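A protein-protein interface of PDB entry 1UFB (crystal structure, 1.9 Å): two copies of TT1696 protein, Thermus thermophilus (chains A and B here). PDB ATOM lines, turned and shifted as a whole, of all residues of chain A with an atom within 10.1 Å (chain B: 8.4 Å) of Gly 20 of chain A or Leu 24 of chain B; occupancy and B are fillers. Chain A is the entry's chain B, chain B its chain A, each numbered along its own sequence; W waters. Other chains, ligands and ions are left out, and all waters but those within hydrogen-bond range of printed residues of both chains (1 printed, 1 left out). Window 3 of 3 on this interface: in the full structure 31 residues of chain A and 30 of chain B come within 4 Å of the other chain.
His 17 of chain A touches Ser 21 of chain B, and with the chains exchanged Ser 21 of chain A touches His 17 of chain B.
His 17 of chain A touches Asp 26 of chain B, and with the chains exchanged Asp 26 of chain A touches His 17 of chain B.
Gly 20 of chain A touches Leu 24 of chain B, and with the chains exchanged Leu 24 of chain A touches Gly 20 of chain B.
Leu 24 of chain B touches its own counterpart, Leu 24 of chain A.
Positions printed for both chains: 17, 18, 19, 20, 21, 22, 23, 24, 25, 26, 27, 29 and 30.
Of the 15 pairs that touch across the chains among the printed residues, 11 have their exchanged pair printed and touching as well.
Water W1 bridges OD2 of Asp 26 of chain B (2.8 Å) and O of Arg 16 of chain A (3.0 Å).
Of chain A, only Gly 20 and Leu 24 come within 4 Å of Leu 24 of chain B.
Of chain B, only His 17 (3.1 Å) comes within 4 Å of Ser 21 of chain A.
Of the printed residues of chain A, Ser 21 of chain B touches His 17 (3.2 Å).
No residue of chain A comes within 4 Å of Gly 23 of chain B.
No residue of chain A comes within 4 Å of Gly 25 of chain B.
Of the printed residues of chain A, Gly 20 of chain B touches Leu 24.
Printed residues of chain A within 4 Å of Trp 29 of chain B: His 13, Asn 14, His 17, Trp 29 and Ala 33.
Leu 15 of chain A touches none of the printed residues of chain B.
The nearest residue of chain B that does not touch Gly 20 of chain A is Asp 26 of chain B (5.6 Å).
The nearest residue of chain A that does not touch Leu 24 of chain B is His 17 of chain A (4.1 Å).
The nearest printed residue of chain B that does not touch His 13 of chain A is Gly 25 of chain B (5.4 Å).
O of His 17 of chain B lies within hydrogen-bond range of OG of Ser 21 of chain B, at 2.6 Å.
O of His 17 of chain A lies within hydrogen-bond range of OG of Ser 21 of chain A (2.6 Å).
O of Ser 21 of chain A sits at hydrogen-bond distance from N of Asp 26 of chain A (2.9 Å).
The backbone carbonyl oxygen (O) of Ser 21 of chain B is in hydrogen-bond range of the backbone NH (N) of Asp 26 of chain B (2.9 Å).
Hydrophobic or aromatic side chains of chain B within 4 Å of the printed part of chain A: His 17, Leu 24 and Trp 29.
Along chain B the printed residues that touch a printed residue of chain A span positions 17 to 29.
Of the 25 printed residues of chain A, 9 touch a printed residue of chain B.
Among the printed residues, pairs that only touch across the chains: Ser 21 of chain A with His 17 of chain B, His 17 of chain A with Ser 21 of chain B, His 17 of chain A with Trp 29 of chain B, His 13 of chain A with Trp 29 of chain B, Trp 29 of chain A with His 17 of chain B, His 13 of chain A with Asp 26 of chain B, Leu 24 of chain A with Gly 20 of chain B, Gly 20 of chain A with Leu 24 of chain B, Trp 29 of chain A with Trp 29 of chain B, Leu 24 of chain A with Leu 24 of chain B and Ala 33 of chain A with Trp 29 of chain B.
The indole nitrogen (NE1) of Trp 29 of chain B lies within hydrogen-bond range of the side-chain amide oxygen (OD1) of Asn 14 of chain A (3.0 Å).
A ring nitrogen (ND1) of His 17 of chain B is in hydrogen-bond range of the side-chain carboxylate (OD2) of Asp 26 of chain A (2.7 Å).
A ring nitrogen (NE2) of His 17 of chain B lies within hydrogen-bond range of a ring nitrogen (NE2) of His 17 of chain A (2.7 Å).
The side-chain carboxylate of Asp 26 of chain B lies within hydrogen-bond range of a ring nitrogen (ND1) of His 17 of chain A (2.8 Å).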
ATOM      1  N   ARG A  12      19.405  10.577  12.074  1.00  0.00           N
ATOM      2  CA  ARG A  12      19.678  11.888  12.660  1.00  0.00           C
ATOM      3  C   ARG A  12      18.862  12.125  13.925  1.00  0.00           C
ATOM      4  O   ARG A  12      19.367  12.661  14.915  1.00  0.00           O
ATOM      5  CB  ARG A  12      19.435  13.007  11.639  1.00  0.00           C
ATOM      6  CG  ARG A  12      20.447  12.962  10.447  1.00  0.00           C
ATOM      7  CD  ARG A  12      20.420  14.268   9.607  1.00  0.00           C
ATOM      8  NE  ARG A  12      19.136  14.386   8.923  1.00  0.00           N
ATOM      9  CZ  ARG A  12      18.816  13.756   7.790  1.00  0.00           C
ATOM     10  NH1 ARG A  12      19.709  12.968   7.202  1.00  0.00           N
ATOM     11  NH2 ARG A  12      17.592  13.883   7.270  1.00  0.00           N
ATOM     12  N   HIS A  13      17.600  11.722  13.898  1.00  0.00           N
ATOM     13  CA  HIS A  13      16.754  11.860  15.058  1.00  0.00           C
ATOM     14  C   HIS A  13      17.330  11.008  16.225  1.00  0.00           C
ATOM     15  O   HIS A  13      17.337  11.420  17.421  1.00  0.00           O
ATOM     16  CB  HIS A  13      15.327  11.358  14.737  1.00  0.00           C
ATOM     17  CG  HIS A  13      14.392  11.531  15.892  1.00  0.00           C
ATOM     18  ND1 HIS A  13      14.024  10.489  16.721  1.00  0.00           N
ATOM     19  CD2 HIS A  13      13.866  12.649  16.445  1.00  0.00           C
ATOM     20  CE1 HIS A  13      13.318  10.967  17.741  1.00  0.00           C
ATOM     21  NE2 HIS A  13      13.209  12.272  17.594  1.00  0.00           N
ATOM     22  N   ASN A  14      17.770   9.808  15.882  1.00  0.00           N
ATOM     23  CA  ASN A  14      18.364   8.940  16.885  1.00  0.00           C
ATOM     24  C   ASN A  14      19.577   9.618  17.510  1.00  0.00           C
ATOM     25  O   ASN A  14      19.746   9.606  18.743  1.00  0.00           O
ATOM     26  CB  ASN A  14      18.779   7.582  16.310  1.00  0.00           C
ATOM     27  CG  ASN A  14      17.568   6.694  15.985  1.00  0.00           C
ATOM     28  OD1 ASN A  14      16.463   6.973  16.439  1.00  0.00           O
ATOM     29  ND2 ASN A  14      17.789   5.642  15.201  1.00  0.00           N
ATOM     30  N   LEU A  15      20.373  10.281  16.683  1.00  0.00           N
ATOM     31  CA  LEU A  15      21.589  10.930  17.190  1.00  0.00           C
ATOM     32  C   LEU A  15      21.201  12.094  18.088  1.00  0.00           C
ATOM     33  O   LEU A  15      21.802  12.327  19.135  1.00  0.00           O
ATOM     34  CB  LEU A  15      22.488  11.392  16.005  1.00  0.00           C
ATOM     35  CG  LEU A  15      23.834  12.025  16.452  1.00  0.00           C
ATOM     36  CD1 LEU A  15      24.653  11.019  17.268  1.00  0.00           C
ATOM     37  CD2 LEU A  15      24.664  12.415  15.218  1.00  0.00           C
ATOM     38  N   ARG A  16      20.126  12.783  17.719  1.00  0.00           N
ATOM     39  CA  ARG A  16      19.653  13.916  18.527  1.00  0.00           C
ATOM     40  C   ARG A  16      19.089  13.391  19.855  1.00  0.00           C
ATOM     41  O   ARG A  16      19.246  14.041  20.883  1.00  0.00           O
ATOM     42  CB  ARG A  16      18.585  14.672  17.768  1.00  0.00           C
ATOM     43  CG  ARG A  16      19.174  15.577  16.720  1.00  0.00           C
ATOM     44  CD  ARG A  16      18.072  16.192  15.911  1.00  0.00           C
ATOM     45  NE  ARG A  16      18.454  16.159  14.508  1.00  0.00           N
ATOM     46  CZ  ARG A  16      17.663  15.735  13.542  1.00  0.00           C
ATOM     47  NH1 ARG A  16      16.446  15.302  13.837  1.00  0.00           N
ATOM     48  NH2 ARG A  16      18.077  15.789  12.281  1.00  0.00           N
ATOM     49  N   HIS A  17      18.474  12.200  19.837  1.00  0.00           N
ATOM     50  CA  HIS A  17      17.969  11.636  21.092  1.00  0.00           C
ATOM     51  C   HIS A  17      19.170  11.228  21.983  1.00  0.00           C
ATOM     52  O   HIS A  17      19.157  11.336  23.244  1.00  0.00           O
ATOM     53  CB  HIS A  17      17.082  10.397  20.852  1.00  0.00           C
ATOM     54  CG  HIS A  17      16.533   9.836  22.140  1.00  0.00           C
ATOM     55  ND1 HIS A  17      15.739  10.588  22.973  1.00  0.00           N
ATOM     56  CD2 HIS A  17      16.759   8.657  22.784  1.00  0.00           C
ATOM     57  CE1 HIS A  17      15.503   9.907  24.082  1.00  0.00           C
ATOM     58  NE2 HIS A  17      16.107   8.732  23.998  1.00  0.00           N
ATOM     59  N   ALA A  18      20.229  10.775  21.322  1.00  0.00           N
ATOM     60  CA  ALA A  18      21.462  10.403  22.007  1.00  0.00           C
ATOM     61  C   ALA A  18      22.012  11.675  22.707  1.00  0.00           C
ATOM     62  O   ALA A  18      22.363  11.640  23.905  1.00  0.00           O
ATOM     63  CB  ALA A  18      22.499   9.839  20.983  1.00  0.00           C
ATOM     64  N   GLN A  19      22.106  12.791  21.973  1.00  0.00           N
ATOM     65  CA  GLN A  19      22.581  14.045  22.587  1.00  0.00           C
ATOM     66  C   GLN A  19      21.661  14.489  23.762  1.00  0.00           C
ATOM     67  O   GLN A  19      22.147  14.878  24.834  1.00  0.00           O
ATOM     68  CB  GLN A  19      22.645  15.126  21.515  1.00  0.00           C
ATOM     69  CG  GLN A  19      23.473  14.692  20.354  1.00  0.00           C
ATOM     70  CD  GLN A  19      23.458  15.668  19.170  1.00  0.00           C
ATOM     71  OE1 GLN A  19      22.386  16.096  18.714  1.00  0.00           O
ATOM     72  NE2 GLN A  19      24.649  15.993  18.652  1.00  0.00           N
ATOM     73  N   GLY A  20      20.332  14.411  23.591  1.00  0.00           N
ATOM     74  CA  GLY A  20      19.467  14.794  24.712  1.00  0.00           C
ATOM     75  C   GLY A  20      19.663  13.907  25.960  1.00  0.00           C
ATOM     76  O   GLY A  20      19.636  14.350  27.148  1.00  0.00           O
ATOM     77  N   SER A  21      19.875  12.618  25.683  1.00  0.00           N
ATOM     78  CA  SER A  21      20.034  11.612  26.716  1.00  0.00           C
ATOM     79  C   SER A  21      21.289  11.950  27.517  1.00  0.00           C
ATOM     80  O   SER A  21      21.295  11.876  28.762  1.00  0.00           O
ATOM     81  CB  SER A  21      20.081  10.174  26.046  1.00  0.00           C
ATOM     82  OG  SER A  21      18.800   9.894  25.382  1.00  0.00           O
ATOM     83  N   LEU A  22      22.321  12.398  26.812  1.00  0.00           N
ATOM     84  CA  LEU A  22      23.566  12.752  27.492  1.00  0.00           C
ATOM     85  C   LEU A  22      23.224  13.912  28.461  1.00  0.00           C
ATOM     86  O   LEU A  22      23.718  13.954  29.603  1.00  0.00           O
ATOM     87  CB  LEU A  22      24.591  13.211  26.467  1.00  0.00           C
ATOM     88  CG  LEU A  22      25.921  13.713  27.045  1.00  0.00           C
ATOM     89  CD1 LEU A  22      26.717  12.600  27.733  1.00  0.00           C
ATOM     90  CD2 LEU A  22      26.704  14.242  25.892  1.00  0.00           C
ATOM     91  N   GLY A  23      22.385  14.829  27.963  1.00  0.00           N
ATOM     92  CA  GLY A  23      21.904  15.973  28.754  1.00  0.00           C
ATOM     93  C   GLY A  23      21.098  15.545  29.971  1.00  0.00           C
ATOM     94  O   GLY A  23      21.175  16.176  31.046  1.00  0.00           O
ATOM     95  N   LEU A  24      20.324  14.466  29.837  1.00  0.00           N
ATOM     96  CA  LEU A  24      19.539  13.960  30.953  1.00  0.00           C
ATOM     97  C   LEU A  24      20.377  13.241  31.981  1.00  0.00           C
ATOM     98  O   LEU A  24      19.877  12.964  33.080  1.00  0.00           O
ATOM     99  CB  LEU A  24      18.457  12.975  30.471  1.00  0.00           C
ATOM    100  CG  LEU A  24      17.326  13.619  29.637  1.00  0.00           C
ATOM    101  CD1 LEU A  24      16.298  12.511  29.296  1.00  0.00           C
ATOM    102  CD2 LEU A  24      16.659  14.771  30.420  1.00  0.00           C
ATOM    103  N   GLY A  25      21.635  12.955  31.640  1.00  0.00           N
ATOM    104  CA  GLY A  25      22.499  12.169  32.510  1.00  0.00           C
ATOM    105  C   GLY A  25      22.217  10.681  32.268  1.00  0.00           C
ATOM    106  O   GLY A  25      22.653   9.814  33.046  1.00  0.00           O
ATOM    107  N   ASP A  26      21.477  10.356  31.190  1.00  0.00           N
ATOM    108  CA  ASP A  26      21.094   8.913  30.945  1.00  0.00           C
ATOM    109  C   ASP A  26      22.147   8.323  29.968  1.00  0.00           C
ATOM    110  O   ASP A  26      21.873   8.150  28.771  1.00  0.00           O
ATOM    111  CB  ASP A  26      19.671   8.854  30.340  1.00  0.00           C
ATOM    112  CG  ASP A  26      18.568   9.220  31.348  1.00  0.00           C
ATOM    113  OD1 ASP A  26      18.833   9.262  32.591  1.00  0.00           O
ATOM    114  OD2 ASP A  26      17.394   9.422  30.910  1.00  0.00           O
ATOM    115  N   TYR A  27      23.345   8.018  30.497  1.00  0.00           N
ATOM    116  CA  TYR A  27      24.445   7.627  29.614  1.00  0.00           C
ATOM    117  C   TYR A  27      24.263   6.342  28.862  1.00  0.00           C
ATOM    118  O   TYR A  27      24.644   6.272  27.671  1.00  0.00           O
ATOM    119  CB  TYR A  27      25.767   7.589  30.370  1.00  0.00           C
ATOM    120  CG  TYR A  27      25.974   8.905  31.109  1.00  0.00           C
ATOM    121  CD1 TYR A  27      26.314   8.921  32.446  1.00  0.00           C
ATOM    122  CD2 TYR A  27      25.753  10.114  30.463  1.00  0.00           C
ATOM    123  CE1 TYR A  27      26.447  10.171  33.139  1.00  0.00           C
ATOM    124  CE2 TYR A  27      25.842  11.333  31.123  1.00  0.00           C
ATOM    125  CZ  TYR A  27      26.194  11.365  32.439  1.00  0.00           C
ATOM    126  OH  TYR A  27      26.341  12.626  33.011  1.00  0.00           O
ATOM    127  N   TRP A  29      21.366   4.991  27.897  1.00  0.00           N
ATOM    128  CA  TRP A  29      20.396   5.276  26.829  1.00  0.00           C
ATOM    129  C   TRP A  29      21.032   6.093  25.713  1.00  0.00           C
ATOM    130  O   TRP A  29      20.739   5.883  24.522  1.00  0.00           O
ATOM    131  CB  TRP A  29      19.155   6.000  27.421  1.00  0.00           C
ATOM    132  CG  TRP A  29      18.128   4.992  27.935  1.00  0.00           C
ATOM    133  CD1 TRP A  29      17.911   4.585  29.252  1.00  0.00           C
ATOM    134  CD2 TRP A  29      17.156   4.319  27.138  1.00  0.00           C
ATOM    135  NE1 TRP A  29      16.852   3.705  29.286  1.00  0.00           N
ATOM    136  CE2 TRP A  29      16.370   3.520  28.012  1.00  0.00           C
ATOM    137  CE3 TRP A  29      16.870   4.317  25.767  1.00  0.00           C
ATOM    138  CZ2 TRP A  29      15.293   2.700  27.551  1.00  0.00           C
ATOM    139  CZ3 TRP A  29      15.780   3.508  25.294  1.00  0.00           C
ATOM    140  CH2 TRP A  29      15.017   2.711  26.199  1.00  0.00           C
ATOM    141  N   ALA A  30      21.958   6.995  26.050  1.00  0.00           N
ATOM    142  CA  ALA A  30      22.664   7.759  25.013  1.00  0.00           C
ATOM    143  C   ALA A  30      23.506   6.773  24.154  1.00  0.00           C
ATOM    144  O   ALA A  30      23.554   6.906  22.953  1.00  0.00           O
ATOM    145  CB  ALA A  30      23.638   8.838  25.658  1.00  0.00           C
ATOM    146  N   CYS A  31      24.179   5.796  24.802  1.00  0.00           N
ATOM    147  CA  CYS A  31      24.992   4.842  24.058  1.00  0.00           C
ATOM    148  C   CYS A  31      24.100   4.000  23.122  1.00  0.00           C
ATOM    149  O   CYS A  31      24.452   3.779  21.921  1.00  0.00           O
ATOM    150  CB  CYS A  31      25.769   3.917  25.021  1.00  0.00           C
ATOM    151  SG  CYS A  31      27.116   4.855  25.835  1.00  0.00           S
ATOM    152  N   ALA A  33      21.138   4.814  21.902  1.00  0.00           N
ATOM    153  CA  ALA A  33      20.615   5.621  20.762  1.00  0.00           C
ATOM    154  C   ALA A  33      21.693   5.864  19.713  1.00  0.00           C
ATOM    155  O   ALA A  33      21.395   5.998  18.538  1.00  0.00           O
ATOM    156  CB  ALA A  33      20.060   6.987  21.281  1.00  0.00           C
ATOM    157  N   ALA A  34      22.958   5.954  20.138  1.00  0.00           N
ATOM    158  CA  ALA A  34      24.046   6.163  19.206  1.00  0.00           C
ATOM    159  C   ALA A  34      24.193   4.931  18.327  1.00  0.00           C
ATOM    160  O   ALA A  34      24.429   5.040  17.127  1.00  0.00           O
ATOM    161  CB  ALA A  34      25.378   6.418  19.964  1.00  0.00           C
ATOM    162  N   ARG A 106      29.591   9.119  31.443  1.00  0.00           N
ATOM    163  CA  ARG A 106      29.454  10.251  30.615  1.00  0.00           C
ATOM    164  C   ARG A 106      30.486  10.186  29.465  1.00  0.00           C
ATOM    165  O   ARG A 106      30.165  10.484  28.322  1.00  0.00           O
ATOM    166  CB  ARG A 106      29.655  11.494  31.479  1.00  0.00           C
ATOM    167  CG  ARG A 106      29.315  12.706  30.734  1.00  0.00           C
ATOM    168  CD  ARG A 106      29.432  14.011  31.590  1.00  0.00           C
ATOM    169  NE  ARG A 106      29.034  15.102  30.699  1.00  0.00           N
ATOM    170  CZ  ARG A 106      27.747  15.457  30.477  1.00  0.00           C
ATOM    171  NH1 ARG A 106      26.747  14.840  31.110  1.00  0.00           N
ATOM    172  NH2 ARG A 106      27.452  16.352  29.537  1.00  0.00           N
ATOM    173  N   ALA A 109      29.415   7.873  26.798  1.00  0.00           N
ATOM    174  CA  ALA A 109      28.338   8.431  26.014  1.00  0.00           C
ATOM    175  C   ALA A 109      28.881   9.490  25.075  1.00  0.00           C
ATOM    176  O   ALA A 109      28.474   9.556  23.898  1.00  0.00           O
ATOM    177  CB  ALA A 109      27.244   8.989  26.935  1.00  0.00           C
ATOM    178  N   LEU A 113      28.571   9.193  20.848  1.00  0.00           N
ATOM    179  CA  LEU A 113      28.014  10.235  19.964  1.00  0.00           C
ATOM    180  C   LEU A 113      28.980  10.493  18.832  1.00  0.00           C
ATOM    181  O   LEU A 113      28.609  10.563  17.651  1.00  0.00           O
ATOM    182  CB  LEU A 113      27.820  11.571  20.675  1.00  0.00           C
ATOM    183  CG  LEU A 113      26.857  11.696  21.835  1.00  0.00           C
ATOM    184  CD1 LEU A 113      26.823  13.142  22.369  1.00  0.00           C
ATOM    185  CD2 LEU A 113      25.501  11.273  21.360  1.00  0.00           C
ATOM    186  N   GLN A 117      28.382   9.823  14.852  1.00  0.00           N
ATOM    187  CA  GLN A 117      28.543  10.992  13.912  1.00  0.00           C
ATOM    188  C   GLN A 117      29.490  10.533  12.804  1.00  0.00           C
ATOM    189  O   GLN A 117      29.186  10.718  11.609  1.00  0.00           O
ATOM    190  CB  GLN A 117      29.135  12.253  14.630  1.00  0.00           C
ATOM    191  CG  GLN A 117      28.170  12.812  15.692  1.00  0.00           C
ATOM    192  CD  GLN A 117      28.691  13.969  16.622  1.00  0.00           C
ATOM    193  OE1 GLN A 117      29.874  14.011  17.048  1.00  0.00           O
ATOM    194  NE2 GLN A 117      27.759  14.878  16.989  1.00  0.00           N
ATOM    195  N   HIS B  17      13.701   7.630  32.084  1.00  0.00           N
ATOM    196  CA  HIS B  17      14.229   8.047  30.772  1.00  0.00           C
ATOM    197  C   HIS B  17      13.018   8.442  29.855  1.00  0.00           C
ATOM    198  O   HIS B  17      13.139   9.384  29.042  1.00  0.00           O
ATOM    199  CB  HIS B  17      15.011   6.937  30.022  1.00  0.00           C
ATOM    200  CG  HIS B  17      15.529   7.410  28.687  1.00  0.00           C
ATOM    201  ND1 HIS B  17      16.519   8.369  28.575  1.00  0.00           N
ATOM    202  CD2 HIS B  17      15.188   7.078  27.426  1.00  0.00           C
ATOM    203  CE1 HIS B  17      16.770   8.590  27.294  1.00  0.00           C
ATOM    204  NE2 HIS B  17      15.984   7.819  26.575  1.00  0.00           N
ATOM    205  N   ALA B  18      11.911   7.698  29.916  1.00  0.00           N
ATOM    206  CA  ALA B  18      10.749   8.052  29.065  1.00  0.00           C
ATOM    207  C   ALA B  18      10.184   9.427  29.505  1.00  0.00           C
ATOM    208  O   ALA B  18       9.752  10.218  28.676  1.00  0.00           O
ATOM    209  CB  ALA B  18       9.594   6.910  29.111  1.00  0.00           C
ATOM    210  N   GLN B  19      10.164   9.688  30.815  1.00  0.00           N
ATOM    211  CA  GLN B  19       9.661  10.970  31.315  1.00  0.00           C
ATOM    212  C   GLN B  19      10.543  12.122  30.840  1.00  0.00           C
ATOM    213  O   GLN B  19      10.054  13.217  30.446  1.00  0.00           O
ATOM    214  CB  GLN B  19       9.656  10.957  32.838  1.00  0.00           C
ATOM    215  CG  GLN B  19       8.475  10.267  33.384  1.00  0.00           C
ATOM    216  CD  GLN B  19       8.245  10.690  34.788  1.00  0.00           C
ATOM    217  OE1 GLN B  19       8.958  10.234  35.717  1.00  0.00           O
ATOM    218  NE2 GLN B  19       7.271  11.613  34.980  1.00  0.00           N
ATOM    219  N   GLY B  20      11.859  11.896  30.867  1.00  0.00           N
ATOM    220  CA  GLY B  20      12.772  12.917  30.407  1.00  0.00           C
ATOM    221  C   GLY B  20      12.683  13.058  28.899  1.00  0.00           C
ATOM    222  O   GLY B  20      12.897  14.152  28.364  1.00  0.00           O
ATOM    223  N   SER B  21      12.339  11.972  28.200  1.00  0.00           N
ATOM    224  CA  SER B  21      12.272  12.023  26.725  1.00  0.00           C
ATOM    225  C   SER B  21      11.077  12.890  26.321  1.00  0.00           C
ATOM    226  O   SER B  21      11.084  13.557  25.309  1.00  0.00           O
ATOM    227  CB  SER B  21      12.117  10.609  26.200  1.00  0.00           C
ATOM    228  OG  SER B  21      13.316   9.871  26.467  1.00  0.00           O
ATOM    229  N   LEU B  22      10.064  12.858  27.169  1.00  0.00           N
ATOM    230  CA  LEU B  22       8.851  13.621  26.965  1.00  0.00           C
ATOM    231  C   LEU B  22       9.298  15.092  27.022  1.00  0.00           C
ATOM    232  O   LEU B  22       8.933  15.867  26.157  1.00  0.00           O
ATOM    233  CB  LEU B  22       7.859  13.228  28.079  1.00  0.00           C
ATOM    234  CG  LEU B  22       6.420  13.762  28.164  1.00  0.00           C
ATOM    235  CD1 LEU B  22       5.609  13.342  26.894  1.00  0.00           C
ATOM    236  CD2 LEU B  22       5.749  13.144  29.448  1.00  0.00           C
ATOM    237  N   GLY B  23      10.146  15.440  28.006  1.00  0.00           N
ATOM    238  CA  GLY B  23      10.649  16.785  28.135  1.00  0.00           C
ATOM    239  C   GLY B  23      11.500  17.199  26.946  1.00  0.00           C
ATOM    240  O   GLY B  23      11.533  18.377  26.607  1.00  0.00           O
ATOM    241  N   LEU B  24      12.225  16.256  26.329  1.00  0.00           N
ATOM    242  CA  LEU B  24      13.042  16.542  25.140  1.00  0.00           C
ATOM    243  C   LEU B  24      12.179  16.666  23.892  1.00  0.00           C
ATOM    244  O   LEU B  24      12.673  17.074  22.816  1.00  0.00           O
ATOM    245  CB  LEU B  24      14.032  15.388  24.841  1.00  0.00           C
ATOM    246  CG  LEU B  24      15.112  15.103  25.911  1.00  0.00           C
ATOM    247  CD1 LEU B  24      15.787  13.786  25.590  1.00  0.00           C
ATOM    248  CD2 LEU B  24      16.168  16.233  25.911  1.00  0.00           C
ATOM    249  N   GLY B  25      10.904  16.300  23.995  1.00  0.00           N
ATOM    250  CA  GLY B  25      10.067  16.307  22.792  1.00  0.00           C
ATOM    251  C   GLY B  25      10.281  15.072  21.890  1.00  0.00           C
ATOM    252  O   GLY B  25       9.804  15.022  20.728  1.00  0.00           O
ATOM    253  N   ASP B  26      10.959  14.036  22.427  1.00  0.00           N
ATOM    254  CA  ASP B  26      11.270  12.814  21.596  1.00  0.00           C
ATOM    255  C   ASP B  26      10.199  11.770  21.948  1.00  0.00           C
ATOM    256  O   ASP B  26      10.448  10.826  22.681  1.00  0.00           O
ATOM    257  CB  ASP B  26      12.690  12.306  21.934  1.00  0.00           C
ATOM    258  CG  ASP B  26      13.788  13.257  21.478  1.00  0.00           C
ATOM    259  OD1 ASP B  26      13.517  14.140  20.615  1.00  0.00           O
ATOM    260  OD2 ASP B  26      14.921  13.117  21.973  1.00  0.00           O
ATOM    261  N   TYR B  27       8.991  11.974  21.376  1.00  0.00           N
ATOM    262  CA  TYR B  27       7.816  11.165  21.688  1.00  0.00           C
ATOM    263  C   TYR B  27       7.904   9.681  21.363  1.00  0.00           C
ATOM    264  O   TYR B  27       7.557   8.862  22.199  1.00  0.00           O
ATOM    265  CB  TYR B  27       6.538  11.828  21.052  1.00  0.00           C
ATOM    266  CG  TYR B  27       6.431  13.312  21.466  1.00  0.00           C
ATOM    267  CD1 TYR B  27       6.135  14.336  20.538  1.00  0.00           C
ATOM    268  CD2 TYR B  27       6.663  13.684  22.798  1.00  0.00           C
ATOM    269  CE1 TYR B  27       6.071  15.745  20.983  1.00  0.00           C
ATOM    270  CE2 TYR B  27       6.618  15.018  23.225  1.00  0.00           C
ATOM    271  CZ  TYR B  27       6.325  16.039  22.346  1.00  0.00           C
ATOM    272  OH  TYR B  27       6.279  17.316  22.938  1.00  0.00           O
ATOM    273  N   TRP B  29      10.629   8.000  21.014  1.00  0.00           N
ATOM    274  CA  TRP B  29      11.605   7.401  21.949  1.00  0.00           C
ATOM    275  C   TRP B  29      10.993   7.232  23.326  1.00  0.00           C
ATOM    276  O   TRP B  29      11.315   6.274  24.025  1.00  0.00           O
ATOM    277  CB  TRP B  29      12.896   8.273  22.036  1.00  0.00           C
ATOM    278  CG  TRP B  29      13.868   7.844  20.961  1.00  0.00           C
ATOM    279  CD1 TRP B  29      14.047   8.420  19.736  1.00  0.00           C
ATOM    280  CD2 TRP B  29      14.767   6.722  21.019  1.00  0.00           C
ATOM    281  NE1 TRP B  29      15.021   7.730  19.012  1.00  0.00           N
ATOM    282  CE2 TRP B  29      15.478   6.680  19.779  1.00  0.00           C
ATOM    283  CE3 TRP B  29      15.053   5.766  21.992  1.00  0.00           C
ATOM    284  CZ2 TRP B  29      16.470   5.695  19.493  1.00  0.00           C
ATOM    285  CZ3 TRP B  29      16.048   4.787  21.711  1.00  0.00           C
ATOM    286  CH2 TRP B  29      16.736   4.769  20.460  1.00  0.00           C
ATOM    287  N   ALA B  30      10.133   8.189  23.754  1.00  0.00           N
ATOM    288  CA  ALA B  30       9.473   8.073  25.048  1.00  0.00           C
ATOM    289  C   ALA B  30       8.569   6.826  25.056  1.00  0.00           C
ATOM    290  O   ALA B  30       8.449   6.119  26.073  1.00  0.00           O
ATOM    291  CB  ALA B  30       8.573   9.367  25.344  1.00  0.00           C
HETATM  292  O   HOH W   1      16.821  15.084  22.405  1.00  0.00           O
